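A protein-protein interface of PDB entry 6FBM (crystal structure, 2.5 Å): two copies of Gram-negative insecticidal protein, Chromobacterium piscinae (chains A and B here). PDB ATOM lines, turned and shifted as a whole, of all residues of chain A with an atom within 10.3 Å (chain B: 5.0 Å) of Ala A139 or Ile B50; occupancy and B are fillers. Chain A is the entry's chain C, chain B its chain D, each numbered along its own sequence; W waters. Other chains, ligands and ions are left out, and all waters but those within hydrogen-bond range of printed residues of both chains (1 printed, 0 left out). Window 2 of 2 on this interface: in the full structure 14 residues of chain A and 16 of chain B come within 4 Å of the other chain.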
ATOM      1  N   PHE A  41      10.599  14.441 -32.950  1.00  0.00           N
ATOM      2  CA  PHE A  41      11.291  15.632 -32.456  1.00  0.00           C
ATOM      3  C   PHE A  41      12.283  16.142 -33.445  1.00  0.00           C
ATOM      4  O   PHE A  41      12.683  15.432 -34.351  1.00  0.00           O
ATOM      5  CB  PHE A  41      12.008  15.311 -31.144  1.00  0.00           C
ATOM      6  CG  PHE A  41      11.134  14.630 -30.144  1.00  0.00           C
ATOM      7  CD1 PHE A  41      10.154  15.331 -29.454  1.00  0.00           C
ATOM      8  CD2 PHE A  41      11.284  13.288 -29.899  1.00  0.00           C
ATOM      9  CE1 PHE A  41       9.356  14.711 -28.546  1.00  0.00           C
ATOM     10  CE2 PHE A  41      10.492  12.662 -28.951  1.00  0.00           C
ATOM     11  CZ  PHE A  41       9.516  13.363 -28.289  1.00  0.00           C
ATOM     12  N   LEU A 135      17.305  11.163 -23.900  1.00  0.00           N
ATOM     13  CA  LEU A 135      16.748  12.427 -24.338  1.00  0.00           C
ATOM     14  C   LEU A 135      16.416  13.341 -23.154  1.00  0.00           C
ATOM     15  O   LEU A 135      16.409  12.888 -22.000  1.00  0.00           O
ATOM     16  CB  LEU A 135      15.439  12.141 -25.092  1.00  0.00           C
ATOM     17  CG  LEU A 135      15.567  11.317 -26.361  1.00  0.00           C
ATOM     18  CD1 LEU A 135      14.194  11.251 -27.018  1.00  0.00           C
ATOM     19  CD2 LEU A 135      16.554  11.923 -27.307  1.00  0.00           C
ATOM     20  N   PRO A 136      16.063  14.607 -23.435  1.00  0.00           N
ATOM     21  CA  PRO A 136      15.435  15.441 -22.427  1.00  0.00           C
ATOM     22  C   PRO A 136      14.106  14.883 -21.943  1.00  0.00           C
ATOM     23  O   PRO A 136      13.501  14.006 -22.587  1.00  0.00           O
ATOM     24  CB  PRO A 136      15.207  16.768 -23.145  1.00  0.00           C
ATOM     25  CG  PRO A 136      16.174  16.797 -24.261  1.00  0.00           C
ATOM     26  CD  PRO A 136      16.252  15.355 -24.688  1.00  0.00           C
ATOM     27  N   GLY A 137      13.639  15.409 -20.808  1.00  0.00           N
ATOM     28  CA  GLY A 137      12.339  15.060 -20.250  1.00  0.00           C
ATOM     29  C   GLY A 137      11.246  15.601 -21.119  1.00  0.00           C
ATOM     30  O   GLY A 137      11.480  16.486 -21.896  1.00  0.00           O
ATOM     31  N   ALA A 138      10.038  15.079 -20.953  1.00  0.00           N
ATOM     32  CA  ALA A 138       8.843  15.515 -21.705  1.00  0.00           C
ATOM     33  C   ALA A 138       8.691  16.997 -21.779  1.00  0.00           C
ATOM     34  O   ALA A 138       8.371  17.532 -22.839  1.00  0.00           O
ATOM     35  CB  ALA A 138       7.586  14.937 -21.065  1.00  0.00           C
ATOM     36  N   ALA A 139       8.912  17.673 -20.664  1.00  0.00           N
ATOM     37  CA  ALA A 139       8.662  19.113 -20.602  1.00  0.00           C
ATOM     38  C   ALA A 139       9.668  19.902 -21.424  1.00  0.00           C
ATOM     39  O   ALA A 139       9.321  20.970 -21.927  1.00  0.00           O
ATOM     40  CB  ALA A 139       8.644  19.594 -19.152  1.00  0.00           C
ATOM     41  N   THR A 140      10.886  19.403 -21.589  1.00  0.00           N
ATOM     42  CA  THR A 140      11.866  20.055 -22.458  1.00  0.00           C
ATOM     43  C   THR A 140      11.541  19.767 -23.915  1.00  0.00           C
ATOM     44  O   THR A 140      11.652  20.637 -24.786  1.00  0.00           O
ATOM     45  CB  THR A 140      13.275  19.546 -22.132  1.00  0.00           C
ATOM     46  OG1 THR A 140      13.601  19.809 -20.765  1.00  0.00           O
ATOM     47  CG2 THR A 140      14.335  20.155 -23.066  1.00  0.00           C
ATOM     48  N   LEU A 141      11.172  18.513 -24.189  1.00  0.00           N
ATOM     49  CA  LEU A 141      10.858  18.070 -25.546  1.00  0.00           C
ATOM     50  C   LEU A 141       9.619  18.736 -26.128  1.00  0.00           C
ATOM     51  O   LEU A 141       9.490  18.836 -27.349  1.00  0.00           O
ATOM     52  CB  LEU A 141      10.672  16.542 -25.613  1.00  0.00           C
ATOM     53  CG  LEU A 141      11.900  15.681 -25.407  1.00  0.00           C
ATOM     54  CD1 LEU A 141      11.529  14.256 -25.095  1.00  0.00           C
ATOM     55  CD2 LEU A 141      12.795  15.751 -26.603  1.00  0.00           C
ATOM     56  N   ARG A 142       8.738  19.209 -25.255  1.00  0.00           N
ATOM     57  CA  ARG A 142       7.540  19.937 -25.674  1.00  0.00           C
ATOM     58  C   ARG A 142       7.836  21.076 -26.650  1.00  0.00           C
ATOM     59  O   ARG A 142       7.066  21.305 -27.566  1.00  0.00           O
ATOM     60  CB  ARG A 142       6.788  20.458 -24.460  1.00  0.00           C
ATOM     61  CG  ARG A 142       5.317  20.716 -24.668  1.00  0.00           C
ATOM     62  CD  ARG A 142       4.494  20.095 -23.530  1.00  0.00           C
ATOM     63  NE  ARG A 142       4.915  20.617 -22.235  1.00  0.00           N
ATOM     64  CZ  ARG A 142       4.767  19.995 -21.057  1.00  0.00           C
ATOM     65  NH1 ARG A 142       4.158  18.797 -20.957  1.00  0.00           N
ATOM     66  NH2 ARG A 142       5.229  20.552 -19.932  1.00  0.00           N
ATOM     67  N   SER A 143       8.960  21.750 -26.472  1.00  0.00           N
ATOM     68  CA  SER A 143       9.395  22.818 -27.383  1.00  0.00           C
ATOM     69  C   SER A 143      10.223  22.319 -28.594  1.00  0.00           C
ATOM     70  O   SER A 143      10.739  23.132 -29.366  1.00  0.00           O
ATOM     71  CB  SER A 143      10.214  23.881 -26.615  1.00  0.00           C
ATOM     72  OG  SER A 143      11.497  23.381 -26.275  1.00  0.00           O
ATOM     73  N   MET A 144      10.349  21.007 -28.763  1.00  0.00           N
ATOM     74  CA  MET A 144      11.214  20.421 -29.788  1.00  0.00           C
ATOM     75  C   MET A 144      10.439  19.501 -30.729  1.00  0.00           C
ATOM     76  O   MET A 144      11.016  18.631 -31.373  1.00  0.00           O
ATOM     77  CB  MET A 144      12.328  19.610 -29.112  1.00  0.00           C
ATOM     78  CG  MET A 144      13.316  20.463 -28.364  1.00  0.00           C
ATOM     79  SD  MET A 144      14.301  19.463 -27.237  1.00  0.00           S
ATOM     80  CE  MET A 144      15.316  18.415 -28.345  1.00  0.00           C
ATOM     81  N   LEU A 145       9.110  19.651 -30.771  1.00  0.00           N
ATOM     82  CA  LEU A 145       8.270  18.746 -31.541  1.00  0.00           C
ATOM     83  C   LEU A 145       8.392  19.103 -33.026  1.00  0.00           C
ATOM     84  O   LEU A 145       8.562  20.287 -33.377  1.00  0.00           O
ATOM     85  CB  LEU A 145       6.834  18.892 -31.107  1.00  0.00           C
ATOM     86  CG  LEU A 145       6.529  18.591 -29.639  1.00  0.00           C
ATOM     87  CD1 LEU A 145       5.035  18.667 -29.362  1.00  0.00           C
ATOM     88  CD2 LEU A 145       7.053  17.243 -29.166  1.00  0.00           C
ATOM     89  N   ARG A 150       3.362  18.001 -33.545  1.00  0.00           N
ATOM     90  CA  ARG A 150       2.780  19.039 -32.682  1.00  0.00           C
ATOM     91  C   ARG A 150       1.308  19.317 -33.003  1.00  0.00           C
ATOM     92  O   ARG A 150       0.470  19.393 -32.078  1.00  0.00           O
ATOM     93  CB  ARG A 150       3.573  20.344 -32.717  1.00  0.00           C
ATOM     94  CG  ARG A 150       2.968  21.470 -31.848  1.00  0.00           C
ATOM     95  CD  ARG A 150       3.661  22.831 -32.005  1.00  0.00           C
ATOM     96  NE  ARG A 150       5.058  22.746 -31.578  1.00  0.00           N
ATOM     97  CZ  ARG A 150       5.490  22.606 -30.310  1.00  0.00           C
ATOM     98  NH1 ARG A 150       4.632  22.554 -29.277  1.00  0.00           N
ATOM     99  NH2 ARG A 150       6.799  22.512 -30.090  1.00  0.00           N
ATOM    100  N   TYR A 171       7.342   6.678 -26.863  1.00  0.00           N
ATOM    101  CA  TYR A 171       8.529   6.897 -27.656  1.00  0.00           C
ATOM    102  C   TYR A 171       9.777   6.516 -26.885  1.00  0.00           C
ATOM    103  O   TYR A 171       9.756   6.406 -25.653  1.00  0.00           O
ATOM    104  CB  TYR A 171       8.581   8.354 -28.131  1.00  0.00           C
ATOM    105  CG  TYR A 171       8.784   9.354 -27.002  1.00  0.00           C
ATOM    106  CD1 TYR A 171      10.068   9.715 -26.584  1.00  0.00           C
ATOM    107  CD2 TYR A 171       7.683   9.920 -26.349  1.00  0.00           C
ATOM    108  CE1 TYR A 171      10.248  10.606 -25.544  1.00  0.00           C
ATOM    109  CE2 TYR A 171       7.862  10.805 -25.313  1.00  0.00           C
ATOM    110  CZ  TYR A 171       9.134  11.158 -24.905  1.00  0.00           C
ATOM    111  OH  TYR A 171       9.273  12.042 -23.878  1.00  0.00           O
ATOM    112  N   SER A 173      12.871   7.229 -25.124  1.00  0.00           N
ATOM    113  CA  SER A 173      13.500   8.320 -24.413  1.00  0.00           C
ATOM    114  C   SER A 173      14.898   8.000 -23.929  1.00  0.00           C
ATOM    115  O   SER A 173      15.716   8.895 -23.786  1.00  0.00           O
ATOM    116  CB  SER A 173      12.629   8.730 -23.229  1.00  0.00           C
ATOM    117  OG  SER A 173      13.134   9.888 -22.650  1.00  0.00           O
ATOM    118  N   GLN A 281       8.546   6.535 -22.875  1.00  0.00           N
ATOM    119  CA  GLN A 281       7.845   7.662 -22.280  1.00  0.00           C
ATOM    120  C   GLN A 281       6.610   7.917 -23.121  1.00  0.00           C
ATOM    121  O   GLN A 281       6.652   7.764 -24.327  1.00  0.00           O
ATOM    122  CB  GLN A 281       8.746   8.870 -22.241  1.00  0.00           C
ATOM    123  CG  GLN A 281       9.933   8.733 -21.302  1.00  0.00           C
ATOM    124  CD  GLN A 281       9.482   8.509 -19.827  1.00  0.00           C
ATOM    125  OE1 GLN A 281       8.573   9.206 -19.369  1.00  0.00           O
ATOM    126  NE2 GLN A 281      10.101   7.557 -19.123  1.00  0.00           N
ATOM    127  N   PRO A 282       5.483   8.244 -22.474  1.00  0.00           N
ATOM    128  CA  PRO A 282       4.237   8.421 -23.209  1.00  0.00           C
ATOM    129  C   PRO A 282       4.230   9.707 -23.999  1.00  0.00           C
ATOM    130  O   PRO A 282       4.767  10.708 -23.547  1.00  0.00           O
ATOM    131  CB  PRO A 282       3.202   8.554 -22.100  1.00  0.00           C
ATOM    132  CG  PRO A 282       3.949   9.138 -20.959  1.00  0.00           C
ATOM    133  CD  PRO A 282       5.327   8.545 -21.033  1.00  0.00           C
ATOM    134  N   ILE A 283       3.608   9.678 -25.165  1.00  0.00           N
ATOM    135  CA  ILE A 283       3.431  10.902 -25.959  1.00  0.00           C
ATOM    136  C   ILE A 283       2.465  11.857 -25.320  1.00  0.00           C
ATOM    137  O   ILE A 283       2.565  13.058 -25.539  1.00  0.00           O
ATOM    138  CB  ILE A 283       3.016  10.669 -27.433  1.00  0.00           C
ATOM    139  CG1 ILE A 283       1.666   9.966 -27.557  1.00  0.00           C
ATOM    140  CG2 ILE A 283       4.107   9.888 -28.150  1.00  0.00           C
ATOM    141  CD1 ILE A 283       1.088  10.097 -28.950  1.00  0.00           C
ATOM    142  N   TRP A 284       1.524  11.346 -24.538  1.00  0.00           N
ATOM    143  CA  TRP A 284       0.532  12.238 -23.903  1.00  0.00           C
ATOM    144  C   TRP A 284       1.171  13.310 -23.002  1.00  0.00           C
ATOM    145  O   TRP A 284       0.779  14.460 -23.072  1.00  0.00           O
ATOM    146  CB  TRP A 284      -0.584  11.479 -23.188  1.00  0.00           C
ATOM    147  CG  TRP A 284      -0.192  10.432 -22.211  1.00  0.00           C
ATOM    148  CD1 TRP A 284       0.286  10.617 -20.942  1.00  0.00           C
ATOM    149  CD2 TRP A 284      -0.315   9.019 -22.398  1.00  0.00           C
ATOM    150  NE1 TRP A 284       0.481   9.404 -20.335  1.00  0.00           N
ATOM    151  CE2 TRP A 284       0.121   8.405 -21.207  1.00  0.00           C
ATOM    152  CE3 TRP A 284      -0.725   8.208 -23.477  1.00  0.00           C
ATOM    153  CZ2 TRP A 284       0.182   7.020 -21.061  1.00  0.00           C
ATOM    154  CZ3 TRP A 284      -0.685   6.846 -23.338  1.00  0.00           C
ATOM    155  CH2 TRP A 284      -0.220   6.257 -22.128  1.00  0.00           C
ATOM    156  N   ALA A 285       2.211  12.952 -22.254  1.00  0.00           N
ATOM    157  CA  ALA A 285       2.996  13.939 -21.479  1.00  0.00           C
ATOM    158  C   ALA A 285       3.535  15.117 -22.294  1.00  0.00           C
ATOM    159  O   ALA A 285       3.909  16.133 -21.742  1.00  0.00           O
ATOM    160  CB  ALA A 285       4.134  13.249 -20.730  1.00  0.00           C
ATOM    161  N   LEU A 286       3.612  14.985 -23.615  1.00  0.00           N
ATOM    162  CA  LEU A 286       4.050  16.055 -24.521  1.00  0.00           C
ATOM    163  C   LEU A 286       2.958  17.054 -24.916  1.00  0.00           C
ATOM    164  O   LEU A 286       3.249  18.102 -25.510  1.00  0.00           O
ATOM    165  CB  LEU A 286       4.640  15.448 -25.779  1.00  0.00           C
ATOM    166  CG  LEU A 286       5.815  14.489 -25.589  1.00  0.00           C
ATOM    167  CD1 LEU A 286       6.123  13.700 -26.827  1.00  0.00           C
ATOM    168  CD2 LEU A 286       7.017  15.266 -25.197  1.00  0.00           C
ATOM    169  N   ALA A 287       1.708  16.728 -24.649  1.00  0.00           N
ATOM    170  CA  ALA A 287       0.597  17.588 -25.070  1.00  0.00           C
ATOM    171  C   ALA A 287       0.590  18.874 -24.219  1.00  0.00           C
ATOM    172  O   ALA A 287       0.919  18.829 -23.046  1.00  0.00           O
ATOM    173  CB  ALA A 287      -0.721  16.840 -24.950  1.00  0.00           C
ATOM    174  N   ASP A 288       0.237  19.996 -24.839  1.00  0.00           N
ATOM    175  CA  ASP A 288       0.216  21.312 -24.155  1.00  0.00           C
ATOM    176  C   ASP A 288      -0.806  21.380 -23.019  1.00  0.00           C
ATOM    177  O   ASP A 288      -0.469  21.768 -21.901  1.00  0.00           O
ATOM    178  CB  ASP A 288      -0.051  22.467 -25.141  1.00  0.00           C
ATOM    179  CG  ASP A 288       1.120  22.742 -26.067  1.00  0.00           C
ATOM    180  OD1 ASP A 288       2.300  22.479 -25.704  1.00  0.00           O
ATOM    181  OD2 ASP A 288       0.845  23.260 -27.155  1.00  0.00           O
ATOM    182  N   ARG A 293      -3.694  15.722 -22.428  1.00  0.00           N
ATOM    183  CA  ARG A 293      -2.852  14.699 -21.795  1.00  0.00           C
ATOM    184  C   ARG A 293      -3.711  13.601 -21.225  1.00  0.00           C
ATOM    185  O   ARG A 293      -3.375  12.423 -21.324  1.00  0.00           O
ATOM    186  CB  ARG A 293      -2.036  15.272 -20.632  1.00  0.00           C
ATOM    187  CG  ARG A 293      -0.953  16.249 -21.015  1.00  0.00           C
ATOM    188  CD  ARG A 293      -0.353  16.909 -19.785  1.00  0.00           C
ATOM    189  NE  ARG A 293       0.310  18.151 -20.140  1.00  0.00           N
ATOM    190  CZ  ARG A 293       0.766  19.059 -19.275  1.00  0.00           C
ATOM    191  NH1 ARG A 293       0.613  18.902 -17.947  1.00  0.00           N
ATOM    192  NH2 ARG A 293       1.361  20.171 -19.753  1.00  0.00           N
ATOM    193  N   LEU B  13      16.573  28.174 -13.967  1.00  0.00           N
ATOM    194  CA  LEU B  13      15.987  26.991 -13.381  1.00  0.00           C
ATOM    195  C   LEU B  13      16.763  26.711 -12.121  1.00  0.00           C
ATOM    196  O   LEU B  13      17.988  26.545 -12.168  1.00  0.00           O
ATOM    197  CB  LEU B  13      16.145  25.770 -14.303  1.00  0.00           C
ATOM    198  CG  LEU B  13      15.590  24.457 -13.792  1.00  0.00           C
ATOM    199  CD1 LEU B  13      14.079  24.422 -13.946  1.00  0.00           C
ATOM    200  CD2 LEU B  13      16.240  23.290 -14.452  1.00  0.00           C
ATOM    201  N   ASP B  48      17.714  25.762 -23.100  1.00  0.00           N
ATOM    202  CA  ASP B  48      16.418  25.136 -23.326  1.00  0.00           C
ATOM    203  C   ASP B  48      15.488  25.761 -22.331  1.00  0.00           C
ATOM    204  O   ASP B  48      15.932  26.427 -21.359  1.00  0.00           O
ATOM    205  CB  ASP B  48      16.466  23.624 -23.076  1.00  0.00           C
ATOM    206  CG  ASP B  48      16.738  22.811 -24.374  1.00  0.00           C
ATOM    207  OD1 ASP B  48      16.319  23.223 -25.482  1.00  0.00           O
ATOM    208  OD2 ASP B  48      17.385  21.757 -24.311  1.00  0.00           O
ATOM    209  N   SER B  49      14.187  25.641 -22.518  1.00  0.00           N
ATOM    210  CA  SER B  49      13.284  26.045 -21.493  1.00  0.00           C
ATOM    211  C   SER B  49      12.249  25.038 -21.184  1.00  0.00           C
ATOM    212  O   SER B  49      11.934  24.240 -21.980  1.00  0.00           O
ATOM    213  CB  SER B  49      12.734  27.481 -21.692  1.00  0.00           C
ATOM    214  OG  SER B  49      11.995  27.635 -22.817  1.00  0.00           O
ATOM    215  N   ILE B  50      11.693  25.119 -19.975  1.00  0.00           N
ATOM    216  CA  ILE B  50      10.494  24.445 -19.608  1.00  0.00           C
ATOM    217  C   ILE B  50       9.487  25.355 -18.907  1.00  0.00           C
ATOM    218  O   ILE B  50       9.858  26.348 -18.316  1.00  0.00           O
ATOM    219  CB  ILE B  50      10.794  23.244 -18.718  1.00  0.00           C
ATOM    220  CG1 ILE B  50      11.556  23.588 -17.434  1.00  0.00           C
ATOM    221  CG2 ILE B  50      11.505  22.151 -19.495  1.00  0.00           C
ATOM    222  CD1 ILE B  50      11.377  22.540 -16.366  1.00  0.00           C
ATOM    223  N   GLU B  51       8.214  25.013 -19.050  1.00  0.00           N
ATOM    224  CA  GLU B  51       7.112  25.732 -18.439  1.00  0.00           C
ATOM    225  C   GLU B  51       6.643  25.008 -17.165  1.00  0.00           C
ATOM    226  O   GLU B  51       6.364  23.813 -17.194  1.00  0.00           O
ATOM    227  CB  GLU B  51       5.967  25.884 -19.440  1.00  0.00           C
ATOM    228  CG  GLU B  51       5.047  27.067 -19.169  1.00  0.00           C
ATOM    229  CD  GLU B  51       3.592  26.645 -18.914  1.00  0.00           C
ATOM    230  OE1 GLU B  51       2.706  27.093 -19.687  1.00  0.00           O
ATOM    231  OE2 GLU B  51       3.311  25.891 -17.934  1.00  0.00           O
ATOM    232  N   ILE B  52       6.607  25.746 -16.071  1.00  0.00           N
ATOM    233  CA  ILE B  52       6.118  25.257 -14.803  1.00  0.00           C
ATOM    234  C   ILE B  52       5.193  26.303 -14.222  1.00  0.00           C
ATOM    235  O   ILE B  52       5.632  27.396 -13.823  1.00  0.00           O
ATOM    236  CB  ILE B  52       7.285  25.011 -13.823  1.00  0.00           C
ATOM    237  CG1 ILE B  52       8.190  23.893 -14.350  1.00  0.00           C
ATOM    238  CG2 ILE B  52       6.806  24.703 -12.412  1.00  0.00           C
ATOM    239  CD1 ILE B  52       9.451  23.735 -13.555  1.00  0.00           C
ATOM    240  N   ARG B  55       5.166  29.843 -15.803  1.00  0.00           N
ATOM    241  CA  ARG B  55       6.411  30.536 -15.935  1.00  0.00           C
ATOM    242  C   ARG B  55       7.460  29.720 -16.678  1.00  0.00           C
ATOM    243  O   ARG B  55       7.495  28.507 -16.591  1.00  0.00           O
ATOM    244  CB  ARG B  55       6.922  30.890 -14.547  1.00  0.00           C
ATOM    245  CG  ARG B  55       5.996  31.856 -13.831  1.00  0.00           C
ATOM    246  CD  ARG B  55       6.687  32.768 -12.837  1.00  0.00           C
ATOM    247  NE  ARG B  55       5.765  33.768 -12.325  1.00  0.00           N
ATOM    248  CZ  ARG B  55       5.952  34.497 -11.206  1.00  0.00           C
ATOM    249  NH1 ARG B  55       7.035  34.354 -10.433  1.00  0.00           N
ATOM    250  NH2 ARG B  55       5.039  35.387 -10.854  1.00  0.00           N
ATOM    251  N   SER B  56       8.386  30.418 -17.307  1.00  0.00           N
ATOM    252  CA  SER B  56       9.480  29.819 -18.029  1.00  0.00           C
ATOM    253  C   SER B  56      10.744  29.688 -17.184  1.00  0.00           C
ATOM    254  O   SER B  56      11.118  30.569 -16.459  1.00  0.00           O
ATOM    255  CB  SER B  56       9.785  30.614 -19.275  1.00  0.00           C
ATOM    256  OG  SER B  56       8.776  30.353 -20.230  1.00  0.00           O
ATOM    257  N   TYR B  57      11.364  28.542 -17.304  1.00  0.00           N
ATOM    258  CA  TYR B  57      12.609  28.270 -16.660  1.00  0.00           C
ATOM    259  C   TYR B  57      13.598  27.842 -17.711  1.00  0.00           C
ATOM    260  O   TYR B  57      13.257  27.082 -18.595  1.00  0.00           O
ATOM    261  CB  TYR B  57      12.433  27.222 -15.603  1.00  0.00           C
ATOM    262  CG  TYR B  57      11.642  27.702 -14.421  1.00  0.00           C
ATOM    263  CD1 TYR B  57      12.333  28.193 -13.402  1.00  0.00           C
ATOM    264  CD2 TYR B  57      10.249  27.511 -14.241  1.00  0.00           C
ATOM    265  CE1 TYR B  57      11.717  28.605 -12.196  1.00  0.00           C
ATOM    266  CE2 TYR B  57       9.598  28.027 -13.159  1.00  0.00           C
ATOM    267  CZ  TYR B  57      10.347  28.534 -12.100  1.00  0.00           C
ATOM    268  OH  TYR B  57       9.749  28.960 -10.942  1.00  0.00           O
ATOM    269  N   PHE B  59      17.711  26.708 -18.793  1.00  0.00           N
ATOM    270  CA  PHE B  59      18.880  25.987 -18.310  1.00  0.00           C
ATOM    271  C   PHE B  59      19.697  25.647 -19.539  1.00  0.00           C
ATOM    272  O   PHE B  59      19.171  25.696 -20.656  1.00  0.00           O
ATOM    273  CB  PHE B  59      18.455  24.726 -17.561  1.00  0.00           C
ATOM    274  CG  PHE B  59      17.615  23.809 -18.354  1.00  0.00           C
ATOM    275  CD1 PHE B  59      16.240  24.009 -18.443  1.00  0.00           C
ATOM    276  CD2 PHE B  59      18.183  22.742 -19.032  1.00  0.00           C
ATOM    277  CE1 PHE B  59      15.434  23.158 -19.196  1.00  0.00           C
ATOM    278  CE2 PHE B  59      17.385  21.884 -19.777  1.00  0.00           C
ATOM    279  CZ  PHE B  59      16.005  22.104 -19.871  1.00  0.00           C
ATOM    280  N   VAL B  65      16.673  17.916 -18.098  1.00  0.00           N
ATOM    281  CA  VAL B  65      15.779  18.131 -17.012  1.00  0.00           C
ATOM    282  C   VAL B  65      14.626  17.172 -17.157  1.00  0.00           C
ATOM    283  O   VAL B  65      14.010  17.072 -18.216  1.00  0.00           O
ATOM    284  CB  VAL B  65      15.281  19.581 -17.006  1.00  0.00           C
ATOM    285  CG1 VAL B  65      14.187  19.785 -15.982  1.00  0.00           C
ATOM    286  CG2 VAL B  65      16.438  20.470 -16.574  1.00  0.00           C
ATOM    287  N   THR B  67      11.152  16.540 -15.079  1.00  0.00           N
ATOM    288  CA  THR B  67      10.247  16.964 -14.033  1.00  0.00           C
ATOM    289  C   THR B  67       9.618  15.708 -13.441  1.00  0.00           C
ATOM    290  O   THR B  67       9.288  14.766 -14.164  1.00  0.00           O
ATOM    291  CB  THR B  67       9.126  17.893 -14.546  1.00  0.00           C
ATOM    292  OG1 THR B  67       8.178  17.159 -15.348  1.00  0.00           O
ATOM    293  CG2 THR B  67       9.705  19.054 -15.287  1.00  0.00           C
HETATM  294  O   HOH W   1       6.772  22.838 -20.123  1.00  0.00           O
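The backbone carbonyl oxygen (O) of Ile B50 lies within hydrogen-bond range of the backbone NH (N) of Tyr B57 (2.8 Å).
The backbone carbonyl oxygen (O) of Thr A140 sits at hydrogen-bond distance from the side-chain hydroxyl (OG) of Ser A143 (3.1 Å).
N of Asp B48 sits at hydrogen-bond distance from O of Phe B59, 2.8 Å away.
O of Val B65 sits at hydrogen-bond distance from N of Gly A137 (3.1 Å).
Hydrophobic or aromatic side chains of chain B that line the printed part of chain A: Ile B50 and Phe B59.
Hydrophobic or aromatic side chains of chain A within 4 Å of the printed part of chain B: Ala A139.
Among the printed residues, 6 pairs touch across the chains.
Water W1 bridges NH2 of Arg A142 (2.8 Å) and N of Glu B51 (2.8 Å).
Of chain B, only Ile B50 (3.5 Å) comes within 4 Å of Ala A139.
Ser B49 touches none of the printed residues of chain A.
No residue of chain A comes within 4 Å of Ser B56.
Of the printed residues of chain A, Val B65 touches Gly A137 and Thr A140.
Of the printed residues of chain B, Thr A140 touches Asp B48 (3.7 Å), Ile B50 (3.4 Å), Phe B59 (3.4 Å) and Val B65 (3.8 Å).
Of the printed residues of chain B, Gly A137 touches Val B65 (3.1 Å).
The nearest residue of chain B that does not touch Ala A139 is Thr B67 (4.04 Å).
Among the printed residues, pairs that only touch across the chains: Ala A139 with Ile B50, Thr A140 with Asp B48, Thr A140 with Ile B50, Thr A140 with Phe B59 and Thr A140 with Val B65.
No position is printed for both chains.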
